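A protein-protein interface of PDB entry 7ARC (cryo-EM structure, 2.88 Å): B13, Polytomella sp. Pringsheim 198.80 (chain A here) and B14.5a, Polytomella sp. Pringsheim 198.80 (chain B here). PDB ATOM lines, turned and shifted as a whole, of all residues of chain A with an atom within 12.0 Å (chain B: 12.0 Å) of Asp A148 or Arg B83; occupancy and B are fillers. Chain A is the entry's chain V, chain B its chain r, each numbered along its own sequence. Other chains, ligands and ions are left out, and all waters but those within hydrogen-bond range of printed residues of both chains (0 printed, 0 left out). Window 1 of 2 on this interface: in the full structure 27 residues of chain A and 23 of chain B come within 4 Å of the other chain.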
ATOM      1  N   ASP A 141       1.042  13.046   8.788  1.00  0.00           N
ATOM      2  CA  ASP A 141      -0.027  12.326   9.469  1.00  0.00           C
ATOM      3  C   ASP A 141      -0.988  11.666   8.486  1.00  0.00           C
ATOM      4  O   ASP A 141      -2.105  11.301   8.867  1.00  0.00           O
ATOM      5  CB  ASP A 141      -0.783  13.261  10.417  1.00  0.00           C
ATOM      6  CG  ASP A 141      -1.469  14.408   9.693  1.00  0.00           C
ATOM      7  OD1 ASP A 141      -1.331  14.517   8.456  1.00  0.00           O
ATOM      8  OD2 ASP A 141      -2.155  15.205  10.366  1.00  0.00           O
ATOM      9  N   TYR A 142      -0.575  11.512   7.230  1.00  0.00           N
ATOM     10  CA  TYR A 142      -1.447  10.945   6.210  1.00  0.00           C
ATOM     11  C   TYR A 142      -1.800   9.503   6.550  1.00  0.00           C
ATOM     12  O   TYR A 142      -0.934   8.711   6.931  1.00  0.00           O
ATOM     13  CB  TYR A 142      -0.766  11.024   4.842  1.00  0.00           C
ATOM     14  CG  TYR A 142      -1.464  10.248   3.748  1.00  0.00           C
ATOM     15  CD1 TYR A 142      -1.072   8.954   3.429  1.00  0.00           C
ATOM     16  CD2 TYR A 142      -2.510  10.810   3.032  1.00  0.00           C
ATOM     17  CE1 TYR A 142      -1.704   8.244   2.432  1.00  0.00           C
ATOM     18  CE2 TYR A 142      -3.149  10.106   2.034  1.00  0.00           C
ATOM     19  CZ  TYR A 142      -2.741   8.823   1.738  1.00  0.00           C
ATOM     20  OH  TYR A 142      -3.373   8.114   0.744  1.00  0.00           O
ATOM     21  N   SER A 143      -3.081   9.166   6.417  1.00  0.00           N
ATOM     22  CA  SER A 143      -3.581   7.841   6.763  1.00  0.00           C
ATOM     23  C   SER A 143      -4.676   7.454   5.783  1.00  0.00           C
ATOM     24  O   SER A 143      -5.691   8.147   5.681  1.00  0.00           O
ATOM     25  CB  SER A 143      -4.112   7.806   8.199  1.00  0.00           C
ATOM     26  OG  SER A 143      -4.628   6.528   8.522  1.00  0.00           O
ATOM     27  N   ALA A 144      -4.468   6.351   5.069  1.00  0.00           N
ATOM     28  CA  ALA A 144      -5.435   5.857   4.096  1.00  0.00           C
ATOM     29  C   ALA A 144      -6.142   4.636   4.663  1.00  0.00           C
ATOM     30  O   ALA A 144      -5.509   3.580   4.820  1.00  0.00           O
ATOM     31  CB  ALA A 144      -4.748   5.510   2.775  1.00  0.00           C
ATOM     32  N   PRO A 145      -7.430   4.723   4.992  1.00  0.00           N
ATOM     33  CA  PRO A 145      -8.128   3.564   5.560  1.00  0.00           C
ATOM     34  C   PRO A 145      -8.285   2.460   4.525  1.00  0.00           C
ATOM     35  O   PRO A 145      -8.663   2.713   3.381  1.00  0.00           O
ATOM     36  CB  PRO A 145      -9.488   4.139   5.971  1.00  0.00           C
ATOM     37  CG  PRO A 145      -9.246   5.599   6.130  1.00  0.00           C
ATOM     38  CD  PRO A 145      -8.240   5.948   5.079  1.00  0.00           C
ATOM     39  N   VAL A 146      -7.989   1.230   4.936  1.00  0.00           N
ATOM     40  CA  VAL A 146      -8.044   0.071   4.056  1.00  0.00           C
ATOM     41  C   VAL A 146      -9.002  -0.943   4.660  1.00  0.00           C
ATOM     42  O   VAL A 146      -8.850  -1.338   5.821  1.00  0.00           O
ATOM     43  CB  VAL A 146      -6.653  -0.548   3.841  1.00  0.00           C
ATOM     44  CG1 VAL A 146      -6.782  -1.980   3.367  1.00  0.00           C
ATOM     45  CG2 VAL A 146      -5.881   0.267   2.833  1.00  0.00           C
ATOM     46  N   PHE A 147      -9.982  -1.363   3.867  1.00  0.00           N
ATOM     47  CA  PHE A 147     -10.975  -2.347   4.269  1.00  0.00           C
ATOM     48  C   PHE A 147     -10.693  -3.659   3.555  1.00  0.00           C
ATOM     49  O   PHE A 147     -10.517  -3.678   2.332  1.00  0.00           O
ATOM     50  CB  PHE A 147     -12.384  -1.851   3.950  1.00  0.00           C
ATOM     51  CG  PHE A 147     -12.817  -0.690   4.795  1.00  0.00           C
ATOM     52  CD1 PHE A 147     -12.417   0.598   4.480  1.00  0.00           C
ATOM     53  CD2 PHE A 147     -13.611  -0.882   5.911  1.00  0.00           C
ATOM     54  CE1 PHE A 147     -12.805   1.669   5.255  1.00  0.00           C
ATOM     55  CE2 PHE A 147     -14.003   0.187   6.691  1.00  0.00           C
ATOM     56  CZ  PHE A 147     -13.599   1.464   6.361  1.00  0.00           C
ATOM     57  N   ASP A 148     -10.650  -4.750   4.312  1.00  0.00           N
ATOM     58  CA  ASP A 148     -10.279  -6.056   3.790  1.00  0.00           C
ATOM     59  C   ASP A 148     -11.423  -7.037   4.000  1.00  0.00           C
ATOM     60  O   ASP A 148     -12.128  -6.976   5.011  1.00  0.00           O
ATOM     61  CB  ASP A 148      -9.013  -6.580   4.468  1.00  0.00           C
ATOM     62  CG  ASP A 148      -7.780  -5.785   4.097  1.00  0.00           C
ATOM     63  OD1 ASP A 148      -7.737  -5.231   2.979  1.00  0.00           O
ATOM     64  OD2 ASP A 148      -6.852  -5.710   4.927  1.00  0.00           O
ATOM     65  N   TYR A 149     -11.598  -7.937   3.038  1.00  0.00           N
ATOM     66  CA  TYR A 149     -12.696  -8.895   3.028  1.00  0.00           C
ATOM     67  C   TYR A 149     -12.233 -10.235   3.585  1.00  0.00           C
ATOM     68  O   TYR A 149     -11.203 -10.768   3.160  1.00  0.00           O
ATOM     69  CB  TYR A 149     -13.226  -9.066   1.606  1.00  0.00           C
ATOM     70  CG  TYR A 149     -14.146 -10.246   1.395  1.00  0.00           C
ATOM     71  CD1 TYR A 149     -15.470 -10.201   1.807  1.00  0.00           C
ATOM     72  CD2 TYR A 149     -13.693 -11.396   0.767  1.00  0.00           C
ATOM     73  CE1 TYR A 149     -16.315 -11.273   1.606  1.00  0.00           C
ATOM     74  CE2 TYR A 149     -14.529 -12.473   0.565  1.00  0.00           C
ATOM     75  CZ  TYR A 149     -15.838 -12.406   0.985  1.00  0.00           C
ATOM     76  OH  TYR A 149     -16.673 -13.481   0.782  1.00  0.00           O
ATOM     77  N   VAL A 150     -12.994 -10.772   4.533  1.00  0.00           N
ATOM     78  CA  VAL A 150     -12.717 -12.067   5.147  1.00  0.00           C
ATOM     79  C   VAL A 150     -13.767 -13.053   4.657  1.00  0.00           C
ATOM     80  O   VAL A 150     -14.971 -12.821   4.817  1.00  0.00           O
ATOM     81  CB  VAL A 150     -12.715 -11.982   6.680  1.00  0.00           C
ATOM     82  CG1 VAL A 150     -12.148 -13.259   7.275  1.00  0.00           C
ATOM     83  CG2 VAL A 150     -11.919 -10.773   7.143  1.00  0.00           C
ATOM     84  N   ASP A 151     -13.313 -14.153   4.066  1.00  0.00           N
ATOM     85  CA  ASP A 151     -14.218 -15.139   3.493  1.00  0.00           C
ATOM     86  C   ASP A 151     -14.759 -16.075   4.566  1.00  0.00           C
ATOM     87  O   ASP A 151     -14.043 -16.464   5.493  1.00  0.00           O
ATOM     88  CB  ASP A 151     -13.504 -15.951   2.413  1.00  0.00           C
ATOM     89  CG  ASP A 151     -14.462 -16.541   1.399  1.00  0.00           C
ATOM     90  OD1 ASP A 151     -15.285 -17.396   1.788  1.00  0.00           O
ATOM     91  OD2 ASP A 151     -14.387 -16.155   0.214  1.00  0.00           O
ATOM     92  N   ALA A 152     -16.038 -16.431   4.430  1.00  0.00           N
ATOM     93  CA  ALA A 152     -16.668 -17.344   5.378  1.00  0.00           C
ATOM     94  C   ALA A 152     -16.113 -18.757   5.254  1.00  0.00           C
ATOM     95  O   ALA A 152     -16.132 -19.514   6.231  1.00  0.00           O
ATOM     96  CB  ALA A 152     -18.181 -17.353   5.172  1.00  0.00           C
ATOM     97  N   THR A 154     -13.081 -19.643   5.070  1.00  0.00           N
ATOM     98  CA  THR A 154     -11.937 -19.781   5.966  1.00  0.00           C
ATOM     99  C   THR A 154     -12.373 -20.129   7.386  1.00  0.00           C
ATOM    100  O   THR A 154     -11.807 -21.030   8.012  1.00  0.00           O
ATOM    101  CB  THR A 154     -11.108 -18.497   5.959  1.00  0.00           C
ATOM    102  OG1 THR A 154     -11.887 -17.419   6.493  1.00  0.00           O
ATOM    103  CG2 THR A 154     -10.672 -18.154   4.541  1.00  0.00           C
ATOM    104  N   ILE A 155     -13.381 -19.429   7.910  1.00  0.00           N
ATOM    105  CA  ILE A 155     -13.780 -19.644   9.299  1.00  0.00           C
ATOM    106  C   ILE A 155     -14.578 -20.936   9.459  1.00  0.00           C
ATOM    107  O   ILE A 155     -14.403 -21.662  10.444  1.00  0.00           O
ATOM    108  CB  ILE A 155     -14.555 -18.425   9.839  1.00  0.00           C
ATOM    109  CG1 ILE A 155     -15.847 -18.192   9.053  1.00  0.00           C
ATOM    110  CG2 ILE A 155     -13.681 -17.180   9.804  1.00  0.00           C
ATOM    111  CD1 ILE A 155     -16.766 -17.163   9.672  1.00  0.00           C
ATOM    112  N   ASN B  77     -22.000 -15.386   6.778  1.00  0.00           N
ATOM    113  CA  ASN B  77     -20.841 -15.474   7.658  1.00  0.00           C
ATOM    114  C   ASN B  77     -19.628 -14.714   7.127  1.00  0.00           C
ATOM    115  O   ASN B  77     -18.504 -14.962   7.576  1.00  0.00           O
ATOM    116  CB  ASN B  77     -20.482 -16.940   7.900  1.00  0.00           C
ATOM    117  CG  ASN B  77     -21.249 -17.540   9.059  1.00  0.00           C
ATOM    118  OD1 ASN B  77     -21.561 -16.854  10.031  1.00  0.00           O
ATOM    119  ND2 ASN B  77     -21.559 -18.827   8.959  1.00  0.00           N
ATOM    120  N   ASN B  78     -19.825 -13.799   6.184  1.00  0.00           N
ATOM    121  CA  ASN B  78     -18.747 -12.966   5.670  1.00  0.00           C
ATOM    122  C   ASN B  78     -18.651 -11.667   6.461  1.00  0.00           C
ATOM    123  O   ASN B  78     -19.659 -11.119   6.912  1.00  0.00           O
ATOM    124  CB  ASN B  78     -18.955 -12.661   4.187  1.00  0.00           C
ATOM    125  CG  ASN B  78     -18.913 -13.904   3.326  1.00  0.00           C
ATOM    126  OD1 ASN B  78     -17.879 -14.560   3.215  1.00  0.00           O
ATOM    127  ND2 ASN B  78     -20.040 -14.236   2.712  1.00  0.00           N
ATOM    128  N   SER B  79     -17.423 -11.177   6.630  1.00  0.00           N
ATOM    129  CA  SER B  79     -17.191  -9.943   7.370  1.00  0.00           C
ATOM    130  C   SER B  79     -16.046  -9.165   6.734  1.00  0.00           C
ATOM    131  O   SER B  79     -15.292  -9.683   5.907  1.00  0.00           O
ATOM    132  CB  SER B  79     -16.886 -10.228   8.846  1.00  0.00           C
ATOM    133  OG  SER B  79     -16.630  -9.029   9.555  1.00  0.00           O
ATOM    134  N   TYR B  80     -15.930  -7.898   7.132  1.00  0.00           N
ATOM    135  CA  TYR B  80     -14.911  -6.986   6.625  1.00  0.00           C
ATOM    136  C   TYR B  80     -14.087  -6.448   7.786  1.00  0.00           C
ATOM    137  O   TYR B  80     -14.639  -5.849   8.714  1.00  0.00           O
ATOM    138  CB  TYR B  80     -15.554  -5.833   5.854  1.00  0.00           C
ATOM    139  CG  TYR B  80     -15.550  -6.017   4.356  1.00  0.00           C
ATOM    140  CD1 TYR B  80     -16.539  -6.759   3.729  1.00  0.00           C
ATOM    141  CD2 TYR B  80     -14.556  -5.454   3.571  1.00  0.00           C
ATOM    142  CE1 TYR B  80     -16.542  -6.931   2.363  1.00  0.00           C
ATOM    143  CE2 TYR B  80     -14.550  -5.623   2.205  1.00  0.00           C
ATOM    144  CZ  TYR B  80     -15.544  -6.362   1.606  1.00  0.00           C
ATOM    145  OH  TYR B  80     -15.542  -6.531   0.243  1.00  0.00           O
ATOM    146  N   THR B  81     -12.776  -6.658   7.738  1.00  0.00           N
ATOM    147  CA  THR B  81     -11.882  -6.071   8.725  1.00  0.00           C
ATOM    148  C   THR B  81     -11.362  -4.719   8.234  1.00  0.00           C
ATOM    149  O   THR B  81     -11.556  -4.328   7.083  1.00  0.00           O
ATOM    150  CB  THR B  81     -10.723  -7.018   9.043  1.00  0.00           C
ATOM    151  OG1 THR B  81     -10.037  -6.556  10.213  1.00  0.00           O
ATOM    152  CG2 THR B  81      -9.747  -7.078   7.890  1.00  0.00           C
ATOM    153  N   VAL B  82     -10.700  -3.994   9.135  1.00  0.00           N
ATOM    154  CA  VAL B  82     -10.264  -2.625   8.885  1.00  0.00           C
ATOM    155  C   VAL B  82      -8.778  -2.501   9.194  1.00  0.00           C
ATOM    156  O   VAL B  82      -8.302  -3.014  10.212  1.00  0.00           O
ATOM    157  CB  VAL B  82     -11.073  -1.613   9.726  1.00  0.00           C
ATOM    158  CG1 VAL B  82     -10.543  -0.202   9.531  1.00  0.00           C
ATOM    159  CG2 VAL B  82     -12.547  -1.685   9.376  1.00  0.00           C
ATOM    160  N   ARG B  83      -8.046  -1.818   8.315  1.00  0.00           N
ATOM    161  CA  ARG B  83      -6.663  -1.448   8.573  1.00  0.00           C
ATOM    162  C   ARG B  83      -6.445   0.006   8.177  1.00  0.00           C
ATOM    163  O   ARG B  83      -7.224   0.593   7.423  1.00  0.00           O
ATOM    164  CB  ARG B  83      -5.661  -2.324   7.807  1.00  0.00           C
ATOM    165  CG  ARG B  83      -5.597  -3.764   8.257  1.00  0.00           C
ATOM    166  CD  ARG B  83      -4.517  -4.516   7.498  1.00  0.00           C
ATOM    167  NE  ARG B  83      -4.834  -4.705   6.088  1.00  0.00           N
ATOM    168  CZ  ARG B  83      -4.170  -4.134   5.091  1.00  0.00           C
ATOM    169  NH1 ARG B  83      -3.168  -3.302   5.317  1.00  0.00           N
ATOM    170  NH2 ARG B  83      -4.521  -4.408   3.838  1.00  0.00           N
ATOM    171  N   SER B  84      -5.371   0.583   8.706  1.00  0.00           N
ATOM    172  CA  SER B  84      -4.941   1.930   8.356  1.00  0.00           C
ATOM    173  C   SER B  84      -3.535   1.854   7.781  1.00  0.00           C
ATOM    174  O   SER B  84      -2.648   1.241   8.384  1.00  0.00           O
ATOM    175  CB  SER B  84      -4.975   2.861   9.571  1.00  0.00           C
ATOM    176  OG  SER B  84      -4.527   4.161   9.230  1.00  0.00           O
ATOM    177  N   VAL B  85      -3.333   2.471   6.621  1.00  0.00           N
ATOM    178  CA  VAL B  85      -2.043   2.476   5.943  1.00  0.00           C
ATOM    179  C   VAL B  85      -1.499   3.897   5.946  1.00  0.00           C
ATOM    180  O   VAL B  85      -2.246   4.861   5.748  1.00  0.00           O
ATOM    181  CB  VAL B  85      -2.160   1.925   4.507  1.00  0.00           C
ATOM    182  CG1 VAL B  85      -0.802   1.891   3.831  1.00  0.00           C
ATOM    183  CG2 VAL B  85      -2.755   0.533   4.535  1.00  0.00           C
ATOM    184  N   ASP B  86      -0.194   4.021   6.179  1.00  0.00           N
ATOM    185  CA  ASP B  86       0.471   5.310   6.262  1.00  0.00           C
ATOM    186  C   ASP B  86       1.672   5.338   5.331  1.00  0.00           C
ATOM    187  O   ASP B  86       2.299   4.310   5.067  1.00  0.00           O
ATOM    188  CB  ASP B  86       0.929   5.609   7.690  1.00  0.00           C
ATOM    189  CG  ASP B  86       1.947   4.606   8.192  1.00  0.00           C
ATOM    190  OD1 ASP B  86       1.591   3.417   8.334  1.00  0.00           O
ATOM    191  OD2 ASP B  86       3.102   5.006   8.443  1.00  0.00           O
ATOM    192  N   SER B  87       1.983   6.535   4.835  1.00  0.00           N
ATOM    193  CA  SER B  87       3.103   6.715   3.921  1.00  0.00           C
ATOM    194  C   SER B  87       4.453   6.686   4.627  1.00  0.00           C
ATOM    195  O   SER B  87       5.474   6.468   3.968  1.00  0.00           O
ATOM    196  CB  SER B  87       2.946   8.028   3.154  1.00  0.00           C
ATOM    197  OG  SER B  87       3.045   9.140   4.025  1.00  0.00           O
ATOM    198  N   THR B  89       5.778   4.552   6.826  1.00  0.00           N
ATOM    199  CA  THR B  89       6.410   3.239   6.835  1.00  0.00           C
ATOM    200  C   THR B  89       6.805   2.840   5.420  1.00  0.00           C
ATOM    201  O   THR B  89       5.949   2.833   4.527  1.00  0.00           O
ATOM    202  CB  THR B  89       5.466   2.200   7.432  1.00  0.00           C
ATOM    203  OG1 THR B  89       4.198   2.269   6.769  1.00  0.00           O
ATOM    204  CG2 THR B  89       5.264   2.460   8.916  1.00  0.00           C
ATOM    205  N   PRO B  90       8.070   2.513   5.167  1.00  0.00           N
ATOM    206  CA  PRO B  90       8.485   2.179   3.803  1.00  0.00           C
ATOM    207  C   PRO B  90       7.919   0.842   3.356  1.00  0.00           C
ATOM    208  O   PRO B  90       7.667  -0.057   4.161  1.00  0.00           O
ATOM    209  CB  PRO B  90      10.013   2.135   3.901  1.00  0.00           C
ATOM    210  CG  PRO B  90      10.272   1.749   5.313  1.00  0.00           C
ATOM    211  CD  PRO B  90       9.185   2.409   6.123  1.00  0.00           C
ATOM    212  N   PHE B  91       7.721   0.722   2.047  1.00  0.00           N
ATOM    213  CA  PHE B  91       7.272  -0.535   1.468  1.00  0.00           C
ATOM    214  C   PHE B  91       8.409  -1.549   1.460  1.00  0.00           C
ATOM    215  O   PHE B  91       9.585  -1.199   1.336  1.00  0.00           O
ATOM    216  CB  PHE B  91       6.752  -0.307   0.049  1.00  0.00           C
ATOM    217  CG  PHE B  91       6.090  -1.505  -0.562  1.00  0.00           C
ATOM    218  CD1 PHE B  91       4.922  -2.016  -0.027  1.00  0.00           C
ATOM    219  CD2 PHE B  91       6.627  -2.111  -1.685  1.00  0.00           C
ATOM    220  CE1 PHE B  91       4.310  -3.114  -0.591  1.00  0.00           C
ATOM    221  CE2 PHE B  91       6.018  -3.209  -2.254  1.00  0.00           C
ATOM    222  CZ  PHE B  91       4.859  -3.712  -1.706  1.00  0.00           C
ATOM    223  N   ASP B  92       8.045  -2.821   1.602  1.00  0.00           N
ATOM    224  CA  ASP B  92       9.014  -3.916   1.628  1.00  0.00           C
ATOM    225  C   ASP B  92       9.223  -4.423   0.208  1.00  0.00           C
ATOM    226  O   ASP B  92       8.486  -5.276  -0.287  1.00  0.00           O
ATOM    227  CB  ASP B  92       8.542  -5.029   2.554  1.00  0.00           C
ATOM    228  CG  ASP B  92       9.682  -5.677   3.313  1.00  0.00           C
ATOM    229  OD1 ASP B  92      10.853  -5.329   3.048  1.00  0.00           O
ATOM    230  OD2 ASP B  92       9.408  -6.540   4.173  1.00  0.00           O
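The backbone carbonyl oxygen of Val B85 sits at hydrogen-bond distance from the backbone NH of Ala A144 (2.8 Å).
O of Asp A148 lies within hydrogen-bond range of N of Thr B81 (2.8 Å).
OD2 of Asp A148 lies within salt-bridge range of NE of Arg B83.
N of Val A150 sits at hydrogen-bond distance from O of Ser B79 (2.9 Å).
OD1 of Asn B78 sits at hydrogen-bond distance from N of Ala A152 (2.9 Å).
N of Arg B83 sits at hydrogen-bond distance from O of Val A146.
OG of Ser A143 lies within hydrogen-bond range of OG of Ser B84 (2.5 Å).
The side-chain amide oxygen of Asn B78 lies within hydrogen-bond range of the side-chain hydroxyl of Tyr A149.
The side-chain hydroxyl of Thr A154 is in hydrogen-bond range of the backbone carbonyl oxygen of Asp A151.
OD2 of Asp B86 lies within hydrogen-bond range of N of Thr B89, 3.2 Å away.
Among the printed residues, merely in contact across the chains: Tyr A142 with Asp B86, Ser A143 with Val B85, Ala A144 with Ser B84, Pro A145 with Arg B83, Val A146 with Val B82, Val A146 with Val B85, Phe A147 with Thr B81, Phe A147 with Val B82, Asp A148 with Tyr B80, Tyr A149 with Ser B79, Tyr A149 with Tyr B80, Val A150 with Asn B78, Asp A151 with Asn B78, Ala A152 with Asn B77 and Ile A155 with Asn B77.
Asp A148 touches three residues of chain B.
Ala A144 touches two residues of chain B.
Of chain B, only Arg B83 (3.6 Å) comes within 4 Å of Pro A145.
Of chain B, only Thr B81 (3.5 Å) and Val B82 (3.6 Å) come within 4 Å of Phe A147.
Val A150 touches two residues of chain B.
Ser B79 touches two residues of chain A.
Tyr B80 touches just these residues of chain A: Asp A148 and Tyr A149.
Of the printed residues of chain A, Val B82 touches Val A146 and Phe A147.
Of the printed residues of chain A, Ser B84 touches Ser A143 and Ala A144.
Of chain A, only Ser A143, Ala A144 and Val A146 come within 4 Å of Val B85.
Printed residues of chain B within 4 Å of Ser A143: Ser B84 (2.5 Å) and Val B85 (3.4 Å).
Of the printed residues of chain A, Asn B77 touches Ala A152 and Ile A155.
Of the printed residues of chain B, Ala A152 touches Asn B77 (3.4 Å) and Asn B78 (2.9 Å).
Of the printed residues of chain A, Asp B86 touches Tyr A142.
Ser B87 touches none of the printed residues of chain A.
Thr A154 touches none of the printed residues of chain B.
The nearest residue of chain B that does not touch Asp A148 is Ser B79 (4.3 Å).
The nearest residue of chain A that does not touch Arg B83 is Ala A144 (4.3 Å).
The nearest printed residue of chain A that does not touch Asn B78 is Ile A155 (5.7 Å).
Of the 14 printed residues of chain A, 12 touch a printed residue of chain B.
Of the 15 printed residues of chain B, 10 touch a printed residue of chain A.
Hydrophobic or aromatic side chains of chain B that line the printed part of chain A: Tyr B80, Val B82 and Val B85.
Along chain B the printed residues that touch a printed residue of chain A span positions 77 to 86.
Among the printed residues, Asp or Glu carboxylates within 4 Å of a Lys or Arg side-chain nitrogen of the other chain: Asp A148 with Arg B83 (2.5 Å).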
